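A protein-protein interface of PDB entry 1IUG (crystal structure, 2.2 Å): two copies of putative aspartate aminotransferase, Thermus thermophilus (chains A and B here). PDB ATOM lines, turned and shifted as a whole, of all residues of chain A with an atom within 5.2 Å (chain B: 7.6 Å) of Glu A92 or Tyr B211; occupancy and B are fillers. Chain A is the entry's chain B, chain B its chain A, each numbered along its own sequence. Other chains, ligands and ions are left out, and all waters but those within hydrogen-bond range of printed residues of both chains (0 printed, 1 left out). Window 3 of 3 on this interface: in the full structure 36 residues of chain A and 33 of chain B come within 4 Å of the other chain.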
ATOM      1  N   THR A  61       4.078 -33.314  -9.550  1.00  0.00           N
ATOM      2  CA  THR A  61       3.246 -32.203 -10.005  1.00  0.00           C
ATOM      3  C   THR A  61       4.119 -31.049 -10.513  1.00  0.00           C
ATOM      4  O   THR A  61       3.757 -30.358 -11.474  1.00  0.00           O
ATOM      5  CB  THR A  61       2.317 -31.716  -8.880  1.00  0.00           C
ATOM      6  OG1 THR A  61       1.413 -32.771  -8.529  1.00  0.00           O
ATOM      7  CG2 THR A  61       1.510 -30.503  -9.326  1.00  0.00           C
ATOM      8  N   GLU A  65       4.111 -29.163 -14.204  1.00  0.00           N
ATOM      9  CA  GLU A  65       4.012 -27.721 -14.396  1.00  0.00           C
ATOM     10  C   GLU A  65       5.188 -27.198 -15.220  1.00  0.00           C
ATOM     11  O   GLU A  65       5.003 -26.363 -16.104  1.00  0.00           O
ATOM     12  CB  GLU A  65       3.940 -26.987 -13.048  1.00  0.00           C
ATOM     13  CG  GLU A  65       3.703 -25.481 -13.187  1.00  0.00           C
ATOM     14  CD  GLU A  65       3.666 -24.735 -11.862  1.00  0.00           C
ATOM     15  OE1 GLU A  65       3.211 -25.305 -10.846  1.00  0.00           O
ATOM     16  OE2 GLU A  65       4.080 -23.559 -11.846  1.00  0.00           O
ATOM     17  N   GLU A  88      -7.308 -34.138 -14.720  1.00  0.00           N
ATOM     18  CA  GLU A  88      -7.997 -32.983 -14.254  1.00  0.00           C
ATOM     19  C   GLU A  88      -6.941 -32.078 -13.757  1.00  0.00           C
ATOM     20  O   GLU A  88      -7.176 -30.881 -13.574  1.00  0.00           O
ATOM     21  CB  GLU A  88      -8.945 -33.258 -13.069  1.00  0.00           C
ATOM     22  CG  GLU A  88      -9.208 -32.046 -12.199  1.00  0.00           C
ATOM     23  CD  GLU A  88     -10.089 -31.009 -12.901  1.00  0.00           C
ATOM     24  OE1 GLU A  88      -9.839 -29.786 -12.736  1.00  0.00           O
ATOM     25  OE2 GLU A  88     -11.035 -31.405 -13.623  1.00  0.00           O
ATOM     26  N   ARG A  89      -5.880 -32.512 -13.260  1.00  0.00           N
ATOM     27  CA  ARG A  89      -4.781 -31.697 -12.769  1.00  0.00           C
ATOM     28  C   ARG A  89      -4.014 -31.074 -13.922  1.00  0.00           C
ATOM     29  O   ARG A  89      -3.432 -29.942 -13.726  1.00  0.00           O
ATOM     30  CB  ARG A  89      -3.846 -32.520 -11.886  1.00  0.00           C
ATOM     31  CG  ARG A  89      -2.795 -31.691 -11.161  1.00  0.00           C
ATOM     32  CD  ARG A  89      -2.028 -32.534 -10.155  1.00  0.00           C
ATOM     33  NE  ARG A  89      -2.886 -33.012  -9.075  1.00  0.00           N
ATOM     34  CZ  ARG A  89      -2.470 -33.789  -8.081  1.00  0.00           C
ATOM     35  NH1 ARG A  89      -1.202 -34.178  -8.031  1.00  0.00           N
ATOM     36  NH2 ARG A  89      -3.320 -34.177  -7.140  1.00  0.00           N
ATOM     37  N   PHE A  90      -3.888 -31.712 -15.045  1.00  0.00           N
ATOM     38  CA  PHE A  90      -3.098 -31.209 -16.161  1.00  0.00           C
ATOM     39  C   PHE A  90      -3.853 -30.050 -16.815  1.00  0.00           C
ATOM     40  O   PHE A  90      -3.239 -29.167 -17.436  1.00  0.00           O
ATOM     41  CB  PHE A  90      -2.835 -32.324 -17.177  1.00  0.00           C
ATOM     42  CG  PHE A  90      -1.658 -32.634 -17.689  1.00  0.00           C
ATOM     43  CD1 PHE A  90      -1.417 -33.827 -18.371  1.00  0.00           C
ATOM     44  CD2 PHE A  90      -0.631 -31.715 -17.528  1.00  0.00           C
ATOM     45  CE1 PHE A  90      -0.179 -34.104 -18.876  1.00  0.00           C
ATOM     46  CE2 PHE A  90       0.634 -31.988 -18.053  1.00  0.00           C
ATOM     47  CZ  PHE A  90       0.861 -33.186 -18.727  1.00  0.00           C
ATOM     48  N   TYR A  91      -5.144 -30.063 -16.662  1.00  0.00           N
ATOM     49  CA  TYR A  91      -6.019 -29.011 -17.168  1.00  0.00           C
ATOM     50  C   TYR A  91      -5.842 -27.735 -16.328  1.00  0.00           C
ATOM     51  O   TYR A  91      -5.792 -26.629 -16.874  1.00  0.00           O
ATOM     52  CB  TYR A  91      -7.478 -29.471 -17.113  1.00  0.00           C
ATOM     53  CG  TYR A  91      -8.495 -28.364 -17.317  1.00  0.00           C
ATOM     54  CD1 TYR A  91      -8.648 -27.751 -18.561  1.00  0.00           C
ATOM     55  CD2 TYR A  91      -9.301 -27.926 -16.263  1.00  0.00           C
ATOM     56  CE1 TYR A  91      -9.576 -26.729 -18.753  1.00  0.00           C
ATOM     57  CE2 TYR A  91     -10.236 -26.905 -16.445  1.00  0.00           C
ATOM     58  CZ  TYR A  91     -10.366 -26.311 -17.693  1.00  0.00           C
ATOM     59  OH  TYR A  91     -11.281 -25.298 -17.885  1.00  0.00           O
ATOM     60  N   GLU A  92      -5.756 -27.899 -15.007  1.00  0.00           N
ATOM     61  CA  GLU A  92      -5.590 -26.767 -14.096  1.00  0.00           C
ATOM     62  C   GLU A  92      -4.221 -26.109 -14.262  1.00  0.00           C
ATOM     63  O   GLU A  92      -4.081 -24.896 -14.106  1.00  0.00           O
ATOM     64  CB  GLU A  92      -5.800 -27.202 -12.642  1.00  0.00           C
ATOM     65  CG  GLU A  92      -7.236 -27.611 -12.298  1.00  0.00           C
ATOM     66  CD  GLU A  92      -7.413 -28.054 -10.847  1.00  0.00           C
ATOM     67  OE1 GLU A  92      -6.459 -27.935 -10.046  1.00  0.00           O
ATOM     68  OE2 GLU A  92      -8.517 -28.527 -10.501  1.00  0.00           O
ATOM     69  N   ILE A  93      -3.215 -26.912 -14.592  1.00  0.00           N
ATOM     70  CA  ILE A  93      -1.867 -26.403 -14.796  1.00  0.00           C
ATOM     71  C   ILE A  93      -1.833 -25.568 -16.076  1.00  0.00           C
ATOM     72  O   ILE A  93      -1.257 -24.480 -16.099  1.00  0.00           O
ATOM     73  CB  ILE A  93      -0.849 -27.556 -14.857  1.00  0.00           C
ATOM     74  CG1 ILE A  93      -0.669 -28.148 -13.456  1.00  0.00           C
ATOM     75  CG2 ILE A  93       0.489 -27.073 -15.426  1.00  0.00           C
ATOM     76  CD1 ILE A  93       0.221 -29.371 -13.399  1.00  0.00           C
ATOM     77  N   ALA A  94      -2.486 -26.069 -17.124  1.00  0.00           N
ATOM     78  CA  ALA A  94      -2.552 -25.372 -18.408  1.00  0.00           C
ATOM     79  C   ALA A  94      -3.266 -24.023 -18.249  1.00  0.00           C
ATOM     80  O   ALA A  94      -2.863 -23.026 -18.854  1.00  0.00           O
ATOM     81  CB  ALA A  94      -3.262 -26.234 -19.436  1.00  0.00           C
ATOM     82  N   LEU A  95      -4.323 -23.995 -17.437  1.00  0.00           N
ATOM     83  CA  LEU A  95      -5.060 -22.757 -17.187  1.00  0.00           C
ATOM     84  C   LEU A  95      -4.185 -21.744 -16.456  1.00  0.00           C
ATOM     85  O   LEU A  95      -4.076 -20.592 -16.880  1.00  0.00           O
ATOM     86  CB  LEU A  95      -6.312 -23.012 -16.346  1.00  0.00           C
ATOM     87  CG  LEU A  95      -7.586 -23.514 -17.021  1.00  0.00           C
ATOM     88  CD1 LEU A  95      -8.662 -23.705 -15.962  1.00  0.00           C
ATOM     89  CD2 LEU A  95      -8.051 -22.517 -18.073  1.00  0.00           C
ATOM     90  N   GLU A  96      -3.553 -22.184 -15.367  1.00  0.00           N
ATOM     91  CA  GLU A  96      -2.699 -21.311 -14.565  1.00  0.00           C
ATOM     92  C   GLU A  96      -1.533 -20.775 -15.386  1.00  0.00           C
ATOM     93  O   GLU A  96      -1.061 -19.662 -15.147  1.00  0.00           O
ATOM     94  CB  GLU A  96      -2.192 -22.055 -13.319  1.00  0.00           C
ATOM     95  CG  GLU A  96      -1.574 -21.166 -12.230  1.00  0.00           C
ATOM     96  CD  GLU A  96      -0.120 -20.776 -12.497  1.00  0.00           C
ATOM     97  OE1 GLU A  96       0.643 -21.594 -13.051  1.00  0.00           O
ATOM     98  OE2 GLU A  96       0.266 -19.646 -12.141  1.00  0.00           O
ATOM     99  N   ALA A  97      -1.086 -21.567 -16.358  1.00  0.00           N
ATOM    100  CA  ALA A  97       0.022 -21.195 -17.234  1.00  0.00           C
ATOM    101  C   ALA A  97      -0.368 -20.152 -18.287  1.00  0.00           C
ATOM    102  O   ALA A  97       0.451 -19.783 -19.129  1.00  0.00           O
ATOM    103  CB  ALA A  97       0.594 -22.444 -17.915  1.00  0.00           C
ATOM    104  N   ASN B  70       3.578 -15.084  -3.335  1.00  0.00           N
ATOM    105  CA  ASN B  70       2.359 -15.060  -2.542  1.00  0.00           C
ATOM    106  C   ASN B  70       2.112 -13.858  -1.640  1.00  0.00           C
ATOM    107  O   ASN B  70       1.070 -13.787  -0.990  1.00  0.00           O
ATOM    108  CB  ASN B  70       2.243 -16.357  -1.738  1.00  0.00           C
ATOM    109  CG  ASN B  70       1.986 -17.566  -2.619  1.00  0.00           C
ATOM    110  OD1 ASN B  70       0.857 -18.034  -2.727  1.00  0.00           O
ATOM    111  ND2 ASN B  70       3.034 -18.072  -3.256  1.00  0.00           N
ATOM    112  N   ARG B 209      -0.969 -17.049  -5.526  1.00  0.00           N
ATOM    113  CA  ARG B 209      -0.619 -17.017  -6.938  1.00  0.00           C
ATOM    114  C   ARG B 209       0.408 -18.088  -7.343  1.00  0.00           C
ATOM    115  O   ARG B 209       1.260 -18.487  -6.542  1.00  0.00           O
ATOM    116  CB  ARG B 209      -0.319 -15.548  -7.328  1.00  0.00           C
ATOM    117  CG  ARG B 209       0.529 -15.166  -8.529  1.00  0.00           C
ATOM    118  CD  ARG B 209       1.957 -15.626  -8.470  1.00  0.00           C
ATOM    119  NE  ARG B 209       2.828 -14.634  -9.110  1.00  0.00           N
ATOM    120  CZ  ARG B 209       2.985 -13.377  -8.693  1.00  0.00           C
ATOM    121  NH1 ARG B 209       2.329 -12.934  -7.633  1.00  0.00           N
ATOM    122  NH2 ARG B 209       3.825 -12.571  -9.323  1.00  0.00           N
ATOM    123  N   GLY B 210       0.230 -18.634  -8.547  1.00  0.00           N
ATOM    124  CA  GLY B 210       1.091 -19.697  -9.048  1.00  0.00           C
ATOM    125  C   GLY B 210       0.310 -21.005  -8.972  1.00  0.00           C
ATOM    126  O   GLY B 210      -0.898 -20.977  -8.738  1.00  0.00           O
ATOM    127  N   TYR B 211       0.954 -22.147  -9.210  1.00  0.00           N
ATOM    128  CA  TYR B 211       0.238 -23.423  -9.109  1.00  0.00           C
ATOM    129  C   TYR B 211       0.826 -24.355  -8.045  1.00  0.00           C
ATOM    130  O   TYR B 211       0.224 -24.549  -6.993  1.00  0.00           O
ATOM    131  CB  TYR B 211       0.135 -24.149 -10.459  1.00  0.00           C
ATOM    132  CG  TYR B 211      -0.876 -25.274 -10.406  1.00  0.00           C
ATOM    133  CD1 TYR B 211      -2.244 -25.007 -10.491  1.00  0.00           C
ATOM    134  CD2 TYR B 211      -0.476 -26.592 -10.181  1.00  0.00           C
ATOM    135  CE1 TYR B 211      -3.186 -26.018 -10.345  1.00  0.00           C
ATOM    136  CE2 TYR B 211      -1.411 -27.610 -10.030  1.00  0.00           C
ATOM    137  CZ  TYR B 211      -2.764 -27.313 -10.109  1.00  0.00           C
ATOM    138  OH  TYR B 211      -3.696 -28.306  -9.915  1.00  0.00           O
ATOM    139  N   TYR B 212       1.992 -24.932  -8.324  1.00  0.00           N
ATOM    140  CA  TYR B 212       2.653 -25.832  -7.380  1.00  0.00           C
ATOM    141  C   TYR B 212       2.982 -25.105  -6.084  1.00  0.00           C
ATOM    142  O   TYR B 212       2.900 -25.695  -5.007  1.00  0.00           O
ATOM    143  CB  TYR B 212       3.947 -26.387  -7.978  1.00  0.00           C
ATOM    144  CG  TYR B 212       4.707 -27.350  -7.082  1.00  0.00           C
ATOM    145  CD1 TYR B 212       4.417 -28.718  -7.085  1.00  0.00           C
ATOM    146  CD2 TYR B 212       5.752 -26.903  -6.267  1.00  0.00           C
ATOM    147  CE1 TYR B 212       5.154 -29.621  -6.305  1.00  0.00           C
ATOM    148  CE2 TYR B 212       6.493 -27.792  -5.481  1.00  0.00           C
ATOM    149  CZ  TYR B 212       6.189 -29.151  -5.508  1.00  0.00           C
ATOM    150  OH  TYR B 212       6.929 -30.038  -4.759  1.00  0.00           O
ATOM    151  N   LEU B 213       3.327 -23.822  -6.193  1.00  0.00           N
ATOM    152  CA  LEU B 213       3.685 -23.036  -5.021  1.00  0.00           C
ATOM    153  C   LEU B 213       2.632 -22.041  -4.507  1.00  0.00           C
ATOM    154  O   LEU B 213       2.952 -21.029  -3.877  1.00  0.00           O
ATOM    155  CB  LEU B 213       5.069 -22.397  -5.216  1.00  0.00           C
ATOM    156  CG  LEU B 213       5.352 -21.072  -5.927  1.00  0.00           C
ATOM    157  CD1 LEU B 213       6.772 -21.139  -6.492  1.00  0.00           C
ATOM    158  CD2 LEU B 213       4.353 -20.783  -7.027  1.00  0.00           C
ATOM    159  N   ASP B 214       1.368 -22.350  -4.776  1.00  0.00           N
ATOM    160  CA  ASP B 214       0.234 -21.551  -4.310  1.00  0.00           C
ATOM    161  C   ASP B 214       0.160 -21.861  -2.803  1.00  0.00           C
ATOM    162  O   ASP B 214      -0.136 -22.989  -2.410  1.00  0.00           O
ATOM    163  CB  ASP B 214      -1.039 -22.035  -5.024  1.00  0.00           C
ATOM    164  CG  ASP B 214      -2.309 -21.303  -4.585  1.00  0.00           C
ATOM    165  OD1 ASP B 214      -2.467 -20.951  -3.396  1.00  0.00           O
ATOM    166  OD2 ASP B 214      -3.189 -21.117  -5.446  1.00  0.00           O
ATOM    167  N   LEU B 215       0.455 -20.868  -1.971  1.00  0.00           N
ATOM    168  CA  LEU B 215       0.437 -21.058  -0.525  1.00  0.00           C
ATOM    169  C   LEU B 215      -0.955 -21.170   0.090  1.00  0.00           C
ATOM    170  O   LEU B 215      -1.109 -21.748   1.165  1.00  0.00           O
ATOM    171  CB  LEU B 215       1.269 -19.975   0.168  1.00  0.00           C
ATOM    172  CG  LEU B 215       2.757 -20.300   0.402  1.00  0.00           C
ATOM    173  CD1 LEU B 215       3.346 -21.135  -0.722  1.00  0.00           C
ATOM    174  CD2 LEU B 215       3.546 -19.023   0.604  1.00  0.00           C
ATOM    175  N   ARG B 217      -3.643 -23.002  -1.023  1.00  0.00           N
ATOM    176  CA  ARG B 217      -4.093 -24.365  -0.794  1.00  0.00           C
ATOM    177  C   ARG B 217      -3.159 -25.296  -0.037  1.00  0.00           C
ATOM    178  O   ARG B 217      -3.583 -26.336   0.454  1.00  0.00           O
ATOM    179  CB  ARG B 217      -4.952 -24.997  -1.915  1.00  0.00           C
ATOM    180  CG  ARG B 217      -4.505 -26.262  -2.678  1.00  0.00           C
ATOM    181  CD  ARG B 217      -3.267 -26.163  -3.515  1.00  0.00           C
ATOM    182  NE  ARG B 217      -3.717 -26.331  -4.903  1.00  0.00           N
ATOM    183  CZ  ARG B 217      -3.320 -25.593  -5.937  1.00  0.00           C
ATOM    184  NH1 ARG B 217      -2.428 -24.628  -5.781  1.00  0.00           N
ATOM    185  NH2 ARG B 217      -3.906 -25.743  -7.114  1.00  0.00           N
ATOM    186  N   GLU B 218      -1.919 -24.857   0.156  1.00  0.00           N
ATOM    187  CA  GLU B 218      -0.974 -25.621   0.962  1.00  0.00           C
ATOM    188  C   GLU B 218      -1.396 -25.342   2.409  1.00  0.00           C
ATOM    189  O   GLU B 218      -1.496 -26.259   3.215  1.00  0.00           O
ATOM    190  CB  GLU B 218       0.474 -25.159   0.751  1.00  0.00           C
ATOM    191  CG  GLU B 218       1.176 -25.766  -0.456  1.00  0.00           C
ATOM    192  CD  GLU B 218       1.509 -27.251  -0.306  1.00  0.00           C
ATOM    193  OE1 GLU B 218       1.066 -27.906   0.667  1.00  0.00           O
ATOM    194  OE2 GLU B 218       2.226 -27.773  -1.186  1.00  0.00           O
ATOM    195  N   ALA B 228      -0.638 -30.163  -0.277  1.00  0.00           N
ATOM    196  CA  ALA B 228      -1.296 -30.105  -1.577  1.00  0.00           C
ATOM    197  C   ALA B 228      -0.974 -31.332  -2.424  1.00  0.00           C
ATOM    198  O   ALA B 228      -1.873 -31.949  -2.989  1.00  0.00           O
ATOM    199  CB  ALA B 228      -0.903 -28.834  -2.309  1.00  0.00           C
ATOM    200  N   TRP B 229       0.304 -31.699  -2.479  1.00  0.00           N
ATOM    201  CA  TRP B 229       0.756 -32.851  -3.265  1.00  0.00           C
ATOM    202  C   TRP B 229       1.478 -33.822  -2.330  1.00  0.00           C
ATOM    203  O   TRP B 229       1.450 -33.643  -1.113  1.00  0.00           O
ATOM    204  CB  TRP B 229       1.711 -32.389  -4.376  1.00  0.00           C
ATOM    205  CG  TRP B 229       1.518 -30.950  -4.777  1.00  0.00           C
ATOM    206  CD1 TRP B 229       2.368 -29.906  -4.525  1.00  0.00           C
ATOM    207  CD2 TRP B 229       0.382 -30.389  -5.447  1.00  0.00           C
ATOM    208  NE1 TRP B 229       1.826 -28.733  -4.990  1.00  0.00           N
ATOM    209  CE2 TRP B 229       0.609 -28.999  -5.560  1.00  0.00           C
ATOM    210  CE3 TRP B 229      -0.808 -30.928  -5.962  1.00  0.00           C
ATOM    211  CZ2 TRP B 229      -0.312 -28.136  -6.169  1.00  0.00           C
ATOM    212  CZ3 TRP B 229      -1.723 -30.069  -6.568  1.00  0.00           C
ATOM    213  CH2 TRP B 229      -1.467 -28.688  -6.665  1.00  0.00           C
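OE1 of Glu A92 lies within hydrogen-bond range of OH of Tyr B211, at 2.8 Å.
The side-chain carboxylate (OE1) of Glu A65 lies within hydrogen-bond range of the backbone NH (N) of Tyr B212.
O of Tyr B211 sits at hydrogen-bond distance from NH1 of Arg B217, at 2.9 Å.
O of Tyr B212 sits at hydrogen-bond distance from NE1 of Trp B229, 3.2 Å away.
The side-chain hydroxyl of Thr A61 lies within hydrogen-bond range of the guanidinium group of Arg A89, at 3.0 Å.
Among the printed residues, pairs that only touch across the chains: Thr A61 with Trp B229, Glu A65 with Tyr B211, Arg A89 with Tyr B211, Arg A89 with Trp B229, Ile A93 with Tyr B211, Glu A96 with Gly B210 and Glu A96 with Tyr B211.
Of chain B, only Tyr B211 (2.8 Å) comes within 4 Å of Glu A92.
Of chain A, only Glu A65 (3.3 Å), Arg A89 (3.7 Å), Glu A92 (2.8 Å), Ile A93 (3.5 Å) and Glu A96 (3.7 Å) come within 4 Å of Tyr B211.
Printed residues of chain B within 4 Å of Thr A61: Trp B229 (3.9 Å).
Of the printed residues of chain A, Trp B229 touches Thr A61 (3.9 Å) and Arg A89 (3.9 Å).
Printed residues of chain B within 4 Å of Glu A65: Tyr B211 and Tyr B212.
Asp B214 touches none of the printed residues of chain A.
Hydrophobic or aromatic side chains of chain A within 4 Å of the printed part of chain B: Ile A93.
Of the 12 printed residues of chain B, 4 touch a printed residue of chain A.
Among the printed residues, no Asp or Glu carboxylate lies within 4 Å of a Lys or Arg side-chain nitrogen of the other chain.
No position is printed for both chains.
Of the 9 pairs that touch across the chains among the printed residues, none has its exchanged pair printed and touching as well.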
